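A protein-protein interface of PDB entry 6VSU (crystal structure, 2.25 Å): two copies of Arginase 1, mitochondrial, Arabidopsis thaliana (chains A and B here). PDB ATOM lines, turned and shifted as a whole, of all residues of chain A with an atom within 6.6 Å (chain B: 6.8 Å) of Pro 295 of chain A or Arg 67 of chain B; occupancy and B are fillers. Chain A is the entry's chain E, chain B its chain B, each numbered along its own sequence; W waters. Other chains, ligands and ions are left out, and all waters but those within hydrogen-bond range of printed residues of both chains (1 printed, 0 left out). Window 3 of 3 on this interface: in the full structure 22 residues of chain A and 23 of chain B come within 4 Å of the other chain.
The guanidinium group of Arg 67 of chain B sits close to the guanidinium group of Arg 67 of chain A. The side-chain amide nitrogen of Gln 296 of chain A is in hydrogen-bond range of the side-chain carboxylate of Glu 70 of chain B, at 2.6 Å.
N of Gln 296 of chain A sits at hydrogen-bond distance from OD1 of Asn 294 of chain A, 3.0 Å away.
Pro 66 of chain B touches Phe 63 of chain A (CB to CE1, 3.6 Å). Arg 67 of chain B touches Phe 63 of chain A (NE to CD1, 3.4 Å). Glu 70 of chain B touches Phe 63 of chain A (OE2 to CE2, 3.7 Å). CD1 of Phe 63 of chain B touches NE of Arg 67 of chain A, at 3.6 Å. NH2 of Arg 67 of chain A touches CB of Pro 295 of chain B, 3.9 Å away. Arg 67 of chain B touches Pro 295 of chain A (NH2 to CB, 3.8 Å). NE2 of Gln 296 of chain A touches NH1 of Arg 67 of chain B, at 3.7 Å.
Pro 295 of chain A touches just one residue of chain B: Arg 67 (3.8 Å). Of chain A, only Phe 63, Arg 67, Pro 295 and Gln 296 come within 4 Å of Arg 67 of chain B. Printed residues of chain B within 4 Å of Phe 63 of chain A: Pro 66 (3.6 Å), Arg 67 (3.4 Å) and Glu 70 (3.7 Å). Printed residues of chain A within 4 Å of Glu 70 of chain B: Phe 63 and Gln 296. Printed residues of chain A within 4 Å of Pro 295 of chain B: Arg 67 (3.9 Å). Of the printed residues of chain A, Pro 66 of chain B touches Phe 63 (3.6 Å). The nearest printed residue of chain B that does not touch Pro 295 of chain A is Pro 295 of chain B (8.0 Å). The nearest printed residue of chain B that does not touch Gln 296 of chain A is Pro 66 of chain B (7.2 Å).
Hydrophobic or aromatic side chains of chain A that line the printed part of chain B: Phe 63 and Pro 295. Hydrophobic or aromatic side chains of chain B within 4 Å of the printed part of chain A: Phe 63, Pro 66 and Pro 295. Among the printed residues, no Asp or Glu carboxylate lies within 4 Å of a Lys or Arg side-chain nitrogen of the other chain.
Phe 63 of chain A touches Arg 67 of chain B, and with the chains exchanged Arg 67 of chain A touches Phe 63 of chain B. Arg 67 of chain B touches its own counterpart, Arg 67 of chain A. Arg 67 of chain A touches Pro 295 of chain B, and with the chains exchanged Pro 295 of chain A touches Arg 67 of chain B. Positions printed for both chains: 63, 64, 65, 67, 293, 295 and 298.
Water W1 bridges OE1 of Gln 296 of chain A (2.6 Å) and OE1 of Glu 70 of chain B (2.6 Å).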
ATOM      1  N   GLY A  60     -22.665   1.724 -29.164  1.00  0.00           N
ATOM      2  CA  GLY A  60     -22.621   2.946 -28.344  1.00  0.00           C
ATOM      3  C   GLY A  60     -21.913   4.146 -28.971  1.00  0.00           C
ATOM      4  O   GLY A  60     -22.374   5.263 -28.778  1.00  0.00           O
ATOM      5  N   PRO A  61     -20.799   3.995 -29.715  1.00  0.00           N
ATOM      6  CA  PRO A  61     -20.175   5.135 -30.364  1.00  0.00           C
ATOM      7  C   PRO A  61     -21.084   5.950 -31.270  1.00  0.00           C
ATOM      8  O   PRO A  61     -20.842   7.087 -31.405  1.00  0.00           O
ATOM      9  CB  PRO A  61     -18.978   4.518 -31.134  1.00  0.00           C
ATOM     10  CG  PRO A  61     -18.648   3.321 -30.251  1.00  0.00           C
ATOM     11  CD  PRO A  61     -19.994   2.768 -29.844  1.00  0.00           C
ATOM     12  N   ALA A  62     -22.138   5.386 -31.805  1.00  0.00           N
ATOM     13  CA  ALA A  62     -23.151   6.193 -32.544  1.00  0.00           C
ATOM     14  C   ALA A  62     -23.620   7.399 -31.727  1.00  0.00           C
ATOM     15  O   ALA A  62     -24.121   8.336 -32.387  1.00  0.00           O
ATOM     16  CB  ALA A  62     -24.351   5.374 -32.925  1.00  0.00           C
ATOM     17  N   PHE A  63     -23.544   7.381 -30.377  1.00  0.00           N
ATOM     18  CA  PHE A  63     -24.129   8.451 -29.518  1.00  0.00           C
ATOM     19  C   PHE A  63     -23.034   9.432 -29.093  1.00  0.00           C
ATOM     20  O   PHE A  63     -23.313  10.371 -28.350  1.00  0.00           O
ATOM     21  CB  PHE A  63     -24.837   7.886 -28.278  1.00  0.00           C
ATOM     22  CG  PHE A  63     -25.956   6.947 -28.585  1.00  0.00           C
ATOM     23  CD1 PHE A  63     -27.125   7.412 -29.140  1.00  0.00           C
ATOM     24  CD2 PHE A  63     -25.851   5.595 -28.355  1.00  0.00           C
ATOM     25  CE1 PHE A  63     -28.182   6.550 -29.431  1.00  0.00           C
ATOM     26  CE2 PHE A  63     -26.889   4.731 -28.646  1.00  0.00           C
ATOM     27  CZ  PHE A  63     -28.066   5.209 -29.175  1.00  0.00           C
ATOM     28  N   ALA A  64     -21.790   9.185 -29.469  1.00  0.00           N
ATOM     29  CA  ALA A  64     -20.638   9.929 -28.939  1.00  0.00           C
ATOM     30  C   ALA A  64     -20.604  11.399 -29.366  1.00  0.00           C
ATOM     31  O   ALA A  64     -20.395  12.263 -28.523  1.00  0.00           O
ATOM     32  CB  ALA A  64     -19.393   9.259 -29.330  1.00  0.00           C
ATOM     33  N   PRO A  65     -20.749  11.781 -30.656  1.00  0.00           N
ATOM     34  CA  PRO A  65     -20.393  13.146 -31.029  1.00  0.00           C
ATOM     35  C   PRO A  65     -21.059  14.235 -30.202  1.00  0.00           C
ATOM     36  O   PRO A  65     -20.406  15.183 -29.784  1.00  0.00           O
ATOM     37  CB  PRO A  65     -20.637  13.224 -32.541  1.00  0.00           C
ATOM     38  CG  PRO A  65     -20.506  11.789 -32.986  1.00  0.00           C
ATOM     39  CD  PRO A  65     -21.101  10.972 -31.837  1.00  0.00           C
ATOM     40  N   ARG A  67     -22.065  14.159 -27.074  1.00  0.00           N
ATOM     41  CA  ARG A  67     -21.485  14.098 -25.715  1.00  0.00           C
ATOM     42  C   ARG A  67     -20.097  14.720 -25.737  1.00  0.00           C
ATOM     43  O   ARG A  67     -19.756  15.428 -24.808  1.00  0.00           O
ATOM     44  CB  ARG A  67     -21.389  12.680 -25.174  1.00  0.00           C
ATOM     45  CG  ARG A  67     -22.684  11.903 -25.242  1.00  0.00           C
ATOM     46  CD  ARG A  67     -23.735  12.680 -24.487  1.00  0.00           C
ATOM     47  NE  ARG A  67     -24.961  11.889 -24.362  1.00  0.00           N
ATOM     48  CZ  ARG A  67     -25.269  11.105 -23.341  1.00  0.00           C
ATOM     49  NH1 ARG A  67     -24.434  10.970 -22.323  1.00  0.00           N
ATOM     50  NH2 ARG A  67     -26.422  10.457 -23.359  1.00  0.00           N
ATOM     51  N   GLY A 260     -15.133   4.265 -20.990  1.00  0.00           N
ATOM     52  CA  GLY A 260     -16.265   4.429 -21.906  1.00  0.00           C
ATOM     53  C   GLY A 260     -15.860   3.979 -23.291  1.00  0.00           C
ATOM     54  O   GLY A 260     -15.733   4.854 -24.230  1.00  0.00           O
ATOM     55  N   VAL A 261     -15.580   2.685 -23.429  1.00  0.00           N
ATOM     56  CA  VAL A 261     -15.211   2.081 -24.734  1.00  0.00           C
ATOM     57  C   VAL A 261     -15.962   0.749 -24.834  1.00  0.00           C
ATOM     58  O   VAL A 261     -16.364   0.170 -23.760  1.00  0.00           O
ATOM     59  CB  VAL A 261     -13.688   1.888 -24.838  1.00  0.00           C
ATOM     60  CG1 VAL A 261     -12.945   3.189 -24.775  1.00  0.00           C
ATOM     61  CG2 VAL A 261     -13.170   0.937 -23.770  1.00  0.00           C
ATOM     62  N   GLU A 292     -14.626   5.704 -31.130  1.00  0.00           N
ATOM     63  CA  GLU A 292     -14.857   4.540 -30.241  1.00  0.00           C
ATOM     64  C   GLU A 292     -15.092   5.000 -28.797  1.00  0.00           C
ATOM     65  O   GLU A 292     -15.095   4.114 -27.905  1.00  0.00           O
ATOM     66  CB  GLU A 292     -13.715   3.543 -30.388  1.00  0.00           C
ATOM     67  CG  GLU A 292     -13.750   2.891 -31.772  1.00  0.00           C
ATOM     68  CD  GLU A 292     -14.831   1.854 -32.019  1.00  0.00           C
ATOM     69  OE1 GLU A 292     -15.481   1.450 -30.993  1.00  0.00           O
ATOM     70  OE2 GLU A 292     -14.983   1.376 -33.216  1.00  0.00           O
ATOM     71  N   PHE A 293     -15.343   6.291 -28.546  1.00  0.00           N
ATOM     72  CA  PHE A 293     -15.894   6.694 -27.234  1.00  0.00           C
ATOM     73  C   PHE A 293     -17.328   6.174 -27.194  1.00  0.00           C
ATOM     74  O   PHE A 293     -18.063   6.419 -28.133  1.00  0.00           O
ATOM     75  CB  PHE A 293     -15.834   8.196 -27.055  1.00  0.00           C
ATOM     76  CG  PHE A 293     -16.774   8.749 -26.022  1.00  0.00           C
ATOM     77  CD1 PHE A 293     -16.939   8.109 -24.796  1.00  0.00           C
ATOM     78  CD2 PHE A 293     -17.432   9.943 -26.242  1.00  0.00           C
ATOM     79  CE1 PHE A 293     -17.819   8.618 -23.864  1.00  0.00           C
ATOM     80  CE2 PHE A 293     -18.286  10.468 -25.282  1.00  0.00           C
ATOM     81  CZ  PHE A 293     -18.495   9.786 -24.109  1.00  0.00           C
ATOM     82  N   ASN A 294     -17.623   5.339 -26.221  1.00  0.00           N
ATOM     83  CA  ASN A 294     -18.931   4.680 -26.026  1.00  0.00           C
ATOM     84  C   ASN A 294     -19.582   5.263 -24.769  1.00  0.00           C
ATOM     85  O   ASN A 294     -19.311   4.759 -23.689  1.00  0.00           O
ATOM     86  CB  ASN A 294     -18.811   3.163 -25.892  1.00  0.00           C
ATOM     87  CG  ASN A 294     -20.160   2.512 -25.862  1.00  0.00           C
ATOM     88  OD1 ASN A 294     -21.164   3.162 -25.532  1.00  0.00           O
ATOM     89  ND2 ASN A 294     -20.181   1.254 -26.247  1.00  0.00           N
ATOM     90  N   PRO A 295     -20.462   6.294 -24.893  1.00  0.00           N
ATOM     91  CA  PRO A 295     -21.124   6.930 -23.755  1.00  0.00           C
ATOM     92  C   PRO A 295     -21.900   5.942 -22.865  1.00  0.00           C
ATOM     93  O   PRO A 295     -21.999   6.150 -21.672  1.00  0.00           O
ATOM     94  CB  PRO A 295     -22.126   7.918 -24.351  1.00  0.00           C
ATOM     95  CG  PRO A 295     -21.750   8.058 -25.773  1.00  0.00           C
ATOM     96  CD  PRO A 295     -20.933   6.845 -26.163  1.00  0.00           C
ATOM     97  N   GLN A 296     -22.415   4.859 -23.433  1.00  0.00           N
ATOM     98  CA  GLN A 296     -23.224   3.891 -22.644  1.00  0.00           C
ATOM     99  C   GLN A 296     -22.278   3.042 -21.769  1.00  0.00           C
ATOM    100  O   GLN A 296     -22.799   2.316 -20.958  1.00  0.00           O
ATOM    101  CB  GLN A 296     -24.070   2.991 -23.544  1.00  0.00           C
ATOM    102  CG  GLN A 296     -24.926   3.803 -24.504  1.00  0.00           C
ATOM    103  CD  GLN A 296     -25.846   3.069 -25.463  1.00  0.00           C
ATOM    104  OE1 GLN A 296     -25.352   2.346 -26.361  1.00  0.00           O
ATOM    105  NE2 GLN A 296     -27.170   3.333 -25.307  1.00  0.00           N
ATOM    106  N   ARG A 297     -20.951   3.100 -21.943  1.00  0.00           N
ATOM    107  CA  ARG A 297     -19.988   2.380 -21.083  1.00  0.00           C
ATOM    108  C   ARG A 297     -19.241   3.370 -20.192  1.00  0.00           C
ATOM    109  O   ARG A 297     -18.390   2.922 -19.429  1.00  0.00           O
ATOM    110  CB  ARG A 297     -19.023   1.548 -21.941  1.00  0.00           C
ATOM    111  CG  ARG A 297     -19.645   0.324 -22.613  1.00  0.00           C
ATOM    112  CD  ARG A 297     -20.233  -0.715 -21.677  1.00  0.00           C
ATOM    113  NE  ARG A 297     -19.754  -2.104 -21.824  1.00  0.00           N
ATOM    114  CZ  ARG A 297     -18.445  -2.459 -21.914  1.00  0.00           C
ATOM    115  NH1 ARG A 297     -17.487  -1.533 -21.917  1.00  0.00           N
ATOM    116  NH2 ARG A 297     -18.096  -3.739 -21.992  1.00  0.00           N
ATOM    117  N   ASP A 298     -19.576   4.655 -20.255  1.00  0.00           N
ATOM    118  CA  ASP A 298     -18.884   5.709 -19.472  1.00  0.00           C
ATOM    119  C   ASP A 298     -19.371   5.698 -17.996  1.00  0.00           C
ATOM    120  O   ASP A 298     -20.380   5.097 -17.696  1.00  0.00           O
ATOM    121  CB  ASP A 298     -19.135   7.087 -20.062  1.00  0.00           C
ATOM    122  CG  ASP A 298     -17.971   8.061 -19.857  1.00  0.00           C
ATOM    123  OD1 ASP A 298     -16.971   7.682 -19.165  1.00  0.00           O
ATOM    124  OD2 ASP A 298     -18.084   9.222 -20.371  1.00  0.00           O
ATOM    125  N   THR A 299     -18.648   6.383 -17.137  1.00  0.00           N
ATOM    126  CA  THR A 299     -19.026   6.632 -15.738  1.00  0.00           C
ATOM    127  C   THR A 299     -20.245   7.543 -15.738  1.00  0.00           C
ATOM    128  O   THR A 299     -20.538   8.230 -16.751  1.00  0.00           O
ATOM    129  CB  THR A 299     -17.864   7.273 -14.981  1.00  0.00           C
ATOM    130  OG1 THR A 299     -17.768   8.614 -15.466  1.00  0.00           O
ATOM    131  CG2 THR A 299     -16.569   6.517 -15.215  1.00  0.00           C
ATOM    132  N   PHE B  63     -30.354  15.067 -25.472  1.00  0.00           N
ATOM    133  CA  PHE B  63     -29.740  13.798 -25.948  1.00  0.00           C
ATOM    134  C   PHE B  63     -30.801  12.679 -26.019  1.00  0.00           C
ATOM    135  O   PHE B  63     -30.448  11.580 -26.416  1.00  0.00           O
ATOM    136  CB  PHE B  63     -28.579  13.419 -25.021  1.00  0.00           C
ATOM    137  CG  PHE B  63     -27.487  14.459 -24.895  1.00  0.00           C
ATOM    138  CD1 PHE B  63     -26.581  14.693 -25.902  1.00  0.00           C
ATOM    139  CD2 PHE B  63     -27.359  15.206 -23.752  1.00  0.00           C
ATOM    140  CE1 PHE B  63     -25.585  15.655 -25.778  1.00  0.00           C
ATOM    141  CE2 PHE B  63     -26.340  16.142 -23.611  1.00  0.00           C
ATOM    142  CZ  PHE B  63     -25.463  16.390 -24.631  1.00  0.00           C
ATOM    143  N   ALA B  64     -32.069  12.925 -25.679  1.00  0.00           N
ATOM    144  CA  ALA B  64     -33.016  11.818 -25.458  1.00  0.00           C
ATOM    145  C   ALA B  64     -33.396  11.102 -26.750  1.00  0.00           C
ATOM    146  O   ALA B  64     -33.454   9.878 -26.744  1.00  0.00           O
ATOM    147  CB  ALA B  64     -34.259  12.286 -24.760  1.00  0.00           C
ATOM    148  N   PRO B  65     -33.788  11.797 -27.844  1.00  0.00           N
ATOM    149  CA  PRO B  65     -34.478  11.132 -28.934  1.00  0.00           C
ATOM    150  C   PRO B  65     -33.694   9.973 -29.525  1.00  0.00           C
ATOM    151  O   PRO B  65     -34.279   8.936 -29.760  1.00  0.00           O
ATOM    152  CB  PRO B  65     -34.750  12.238 -29.948  1.00  0.00           C
ATOM    153  CG  PRO B  65     -34.782  13.506 -29.077  1.00  0.00           C
ATOM    154  CD  PRO B  65     -33.682  13.248 -28.058  1.00  0.00           C
ATOM    155  N   PRO B  66     -32.368  10.031 -29.720  1.00  0.00           N
ATOM    156  CA  PRO B  66     -31.676   8.839 -30.180  1.00  0.00           C
ATOM    157  C   PRO B  66     -31.808   7.676 -29.182  1.00  0.00           C
ATOM    158  O   PRO B  66     -31.976   6.562 -29.619  1.00  0.00           O
ATOM    159  CB  PRO B  66     -30.244   9.357 -30.396  1.00  0.00           C
ATOM    160  CG  PRO B  66     -30.415  10.854 -30.638  1.00  0.00           C
ATOM    161  CD  PRO B  66     -31.526  11.233 -29.697  1.00  0.00           C
ATOM    162  N   ARG B  67     -31.792   7.942 -27.878  1.00  0.00           N
ATOM    163  CA  ARG B  67     -31.850   6.864 -26.859  1.00  0.00           C
ATOM    164  C   ARG B  67     -33.238   6.232 -26.848  1.00  0.00           C
ATOM    165  O   ARG B  67     -33.338   5.022 -26.619  1.00  0.00           O
ATOM    166  CB  ARG B  67     -31.504   7.319 -25.444  1.00  0.00           C
ATOM    167  CG  ARG B  67     -30.183   8.029 -25.373  1.00  0.00           C
ATOM    168  CD  ARG B  67     -29.077   7.334 -26.171  1.00  0.00           C
ATOM    169  NE  ARG B  67     -27.764   7.894 -25.829  1.00  0.00           N
ATOM    170  CZ  ARG B  67     -27.074   7.601 -24.723  1.00  0.00           C
ATOM    171  NH1 ARG B  67     -27.574   6.731 -23.838  1.00  0.00           N
ATOM    172  NH2 ARG B  67     -25.887   8.185 -24.525  1.00  0.00           N
ATOM    173  N   ILE B  68     -34.262   7.017 -27.061  1.00  0.00           N
ATOM    174  CA  ILE B  68     -35.650   6.484 -27.086  1.00  0.00           C
ATOM    175  C   ILE B  68     -35.776   5.531 -28.283  1.00  0.00           C
ATOM    176  O   ILE B  68     -36.268   4.366 -28.103  1.00  0.00           O
ATOM    177  CB  ILE B  68     -36.653   7.638 -27.144  1.00  0.00           C
ATOM    178  CG1 ILE B  68     -36.467   8.588 -25.965  1.00  0.00           C
ATOM    179  CG2 ILE B  68     -38.081   7.109 -27.240  1.00  0.00           C
ATOM    180  CD1 ILE B  68     -37.458   9.757 -25.980  1.00  0.00           C
ATOM    181  N   ARG B  69     -35.275   5.943 -29.452  1.00  0.00           N
ATOM    182  CA  ARG B  69     -35.361   5.049 -30.644  1.00  0.00           C
ATOM    183  C   ARG B  69     -34.657   3.740 -30.347  1.00  0.00           C
ATOM    184  O   ARG B  69     -35.192   2.692 -30.671  1.00  0.00           O
ATOM    185  CB  ARG B  69     -34.679   5.621 -31.883  1.00  0.00           C
ATOM    186  CG  ARG B  69     -35.381   6.856 -32.394  1.00  0.00           C
ATOM    187  CD  ARG B  69     -34.700   7.358 -33.670  1.00  0.00           C
ATOM    188  NE  ARG B  69     -35.550   8.467 -34.109  1.00  0.00           N
ATOM    189  CZ  ARG B  69     -35.355   9.749 -33.818  1.00  0.00           C
ATOM    190  NH1 ARG B  69     -34.249  10.132 -33.196  1.00  0.00           N
ATOM    191  NH2 ARG B  69     -36.210  10.659 -34.263  1.00  0.00           N
ATOM    192  N   GLU B  70     -33.456   3.785 -29.782  1.00  0.00           N
ATOM    193  CA  GLU B  70     -32.743   2.529 -29.461  1.00  0.00           C
ATOM    194  C   GLU B  70     -33.675   1.640 -28.618  1.00  0.00           C
ATOM    195  O   GLU B  70     -33.705   0.423 -28.874  1.00  0.00           O
ATOM    196  CB  GLU B  70     -31.424   2.839 -28.754  1.00  0.00           C
ATOM    197  CG  GLU B  70     -30.509   1.645 -28.624  1.00  0.00           C
ATOM    198  CD  GLU B  70     -29.374   1.730 -27.597  1.00  0.00           C
ATOM    199  OE1 GLU B  70     -28.572   0.824 -27.636  1.00  0.00           O
ATOM    200  OE2 GLU B  70     -29.294   2.661 -26.740  1.00  0.00           O
ATOM    201  N   ALA B  71     -34.351   2.179 -27.593  1.00  0.00           N
ATOM    202  CA  ALA B  71     -35.127   1.386 -26.618  1.00  0.00           C
ATOM    203  C   ALA B  71     -36.372   0.785 -27.288  1.00  0.00           C
ATOM    204  O   ALA B  71     -36.732  -0.372 -26.945  1.00  0.00           O
ATOM    205  CB  ALA B  71     -35.480   2.204 -25.410  1.00  0.00           C
ATOM    206  N   ILE B  72     -36.970   1.499 -28.241  1.00  0.00           N
ATOM    207  CA  ILE B  72     -38.153   1.002 -28.980  1.00  0.00           C
ATOM    208  C   ILE B  72     -37.790  -0.340 -29.643  1.00  0.00           C
ATOM    209  O   ILE B  72     -38.611  -1.262 -29.601  1.00  0.00           O
ATOM    210  CB  ILE B  72     -38.642   2.064 -29.988  1.00  0.00           C
ATOM    211  CG1 ILE B  72     -39.208   3.304 -29.311  1.00  0.00           C
ATOM    212  CG2 ILE B  72     -39.657   1.455 -30.928  1.00  0.00           C
ATOM    213  CD1 ILE B  72     -39.401   4.453 -30.252  1.00  0.00           C
ATOM    214  N   PHE B 293     -37.258  13.230 -20.794  1.00  0.00           N
ATOM    215  CA  PHE B 293     -36.345  12.094 -20.518  1.00  0.00           C
ATOM    216  C   PHE B 293     -34.926  12.653 -20.580  1.00  0.00           C
ATOM    217  O   PHE B 293     -34.553  13.221 -21.620  1.00  0.00           O
ATOM    218  CB  PHE B 293     -36.570  10.945 -21.489  1.00  0.00           C
ATOM    219  CG  PHE B 293     -35.497   9.890 -21.554  1.00  0.00           C
ATOM    220  CD1 PHE B 293     -34.866   9.424 -20.402  1.00  0.00           C
ATOM    221  CD2 PHE B 293     -35.112   9.358 -22.773  1.00  0.00           C
ATOM    222  CE1 PHE B 293     -33.864   8.464 -20.484  1.00  0.00           C
ATOM    223  CE2 PHE B 293     -34.097   8.411 -22.856  1.00  0.00           C
ATOM    224  CZ  PHE B 293     -33.466   7.980 -21.716  1.00  0.00           C
ATOM    225  N   PRO B 295     -31.301  11.287 -20.324  1.00  0.00           N
ATOM    226  CA  PRO B 295     -30.429  10.120 -20.307  1.00  0.00           C
ATOM    227  C   PRO B 295     -29.261  10.276 -19.321  1.00  0.00           C
ATOM    228  O   PRO B 295     -28.821   9.306 -18.795  1.00  0.00           O
ATOM    229  CB  PRO B 295     -29.902  10.002 -21.744  1.00  0.00           C
ATOM    230  CG  PRO B 295     -30.860  10.838 -22.587  1.00  0.00           C
ATOM    231  CD  PRO B 295     -31.468  11.860 -21.667  1.00  0.00           C
ATOM    232  N   ASP B 298     -30.282   8.872 -16.067  1.00  0.00           N
ATOM    233  CA  ASP B 298     -30.926   7.544 -16.150  1.00  0.00           C
ATOM    234  C   ASP B 298     -30.049   6.533 -15.417  1.00  0.00           C
ATOM    235  O   ASP B 298     -28.915   6.825 -15.132  1.00  0.00           O
ATOM    236  CB  ASP B 298     -31.108   7.068 -17.586  1.00  0.00           C
ATOM    237  CG  ASP B 298     -32.256   6.088 -17.794  1.00  0.00           C
ATOM    238  OD1 ASP B 298     -32.873   5.657 -16.784  1.00  0.00           O
ATOM    239  OD2 ASP B 298     -32.494   5.723 -18.954  1.00  0.00           O
ATOM    240  N   ALA B 305     -34.997   5.079 -20.435  1.00  0.00           N
ATOM    241  CA  ALA B 305     -35.098   5.011 -21.902  1.00  0.00           C
ATOM    242  C   ALA B 305     -36.226   4.023 -22.233  1.00  0.00           C
ATOM    243  O   ALA B 305     -36.904   4.255 -23.243  1.00  0.00           O
ATOM    244  CB  ALA B 305     -33.772   4.632 -22.563  1.00  0.00           C
ATOM    245  N   MET B 306     -36.377   2.919 -21.469  1.00  0.00           N
ATOM    246  CA  MET B 306     -37.347   1.841 -21.805  1.00  0.00           C
ATOM    247  C   MET B 306     -38.731   2.377 -21.476  1.00  0.00           C
ATOM    248  O   MET B 306     -39.682   2.083 -22.193  1.00  0.00           O
ATOM    249  CB  MET B 306     -37.090   0.532 -21.051  1.00  0.00           C
ATOM    250  CG  MET B 306     -35.760  -0.108 -21.417  1.00  0.00           C
ATOM    251  SD  MET B 306     -35.591  -0.762 -23.161  1.00  0.00           S
ATOM    252  CE  MET B 306     -37.131  -1.641 -23.354  1.00  0.00           C
ATOM    253  N   ALA B 309     -39.605   4.806 -24.146  1.00  0.00           N
ATOM    254  CA  ALA B 309     -39.869   4.025 -25.376  1.00  0.00           C
ATOM    255  C   ALA B 309     -41.257   3.384 -25.293  1.00  0.00           C
ATOM    256  O   ALA B 309     -41.965   3.361 -26.321  1.00  0.00           O
ATOM    257  CB  ALA B 309     -38.806   2.984 -25.639  1.00  0.00           C
HETATM  258  O   HOH W   1     -26.054   0.976 -28.439  1.00  0.00           O
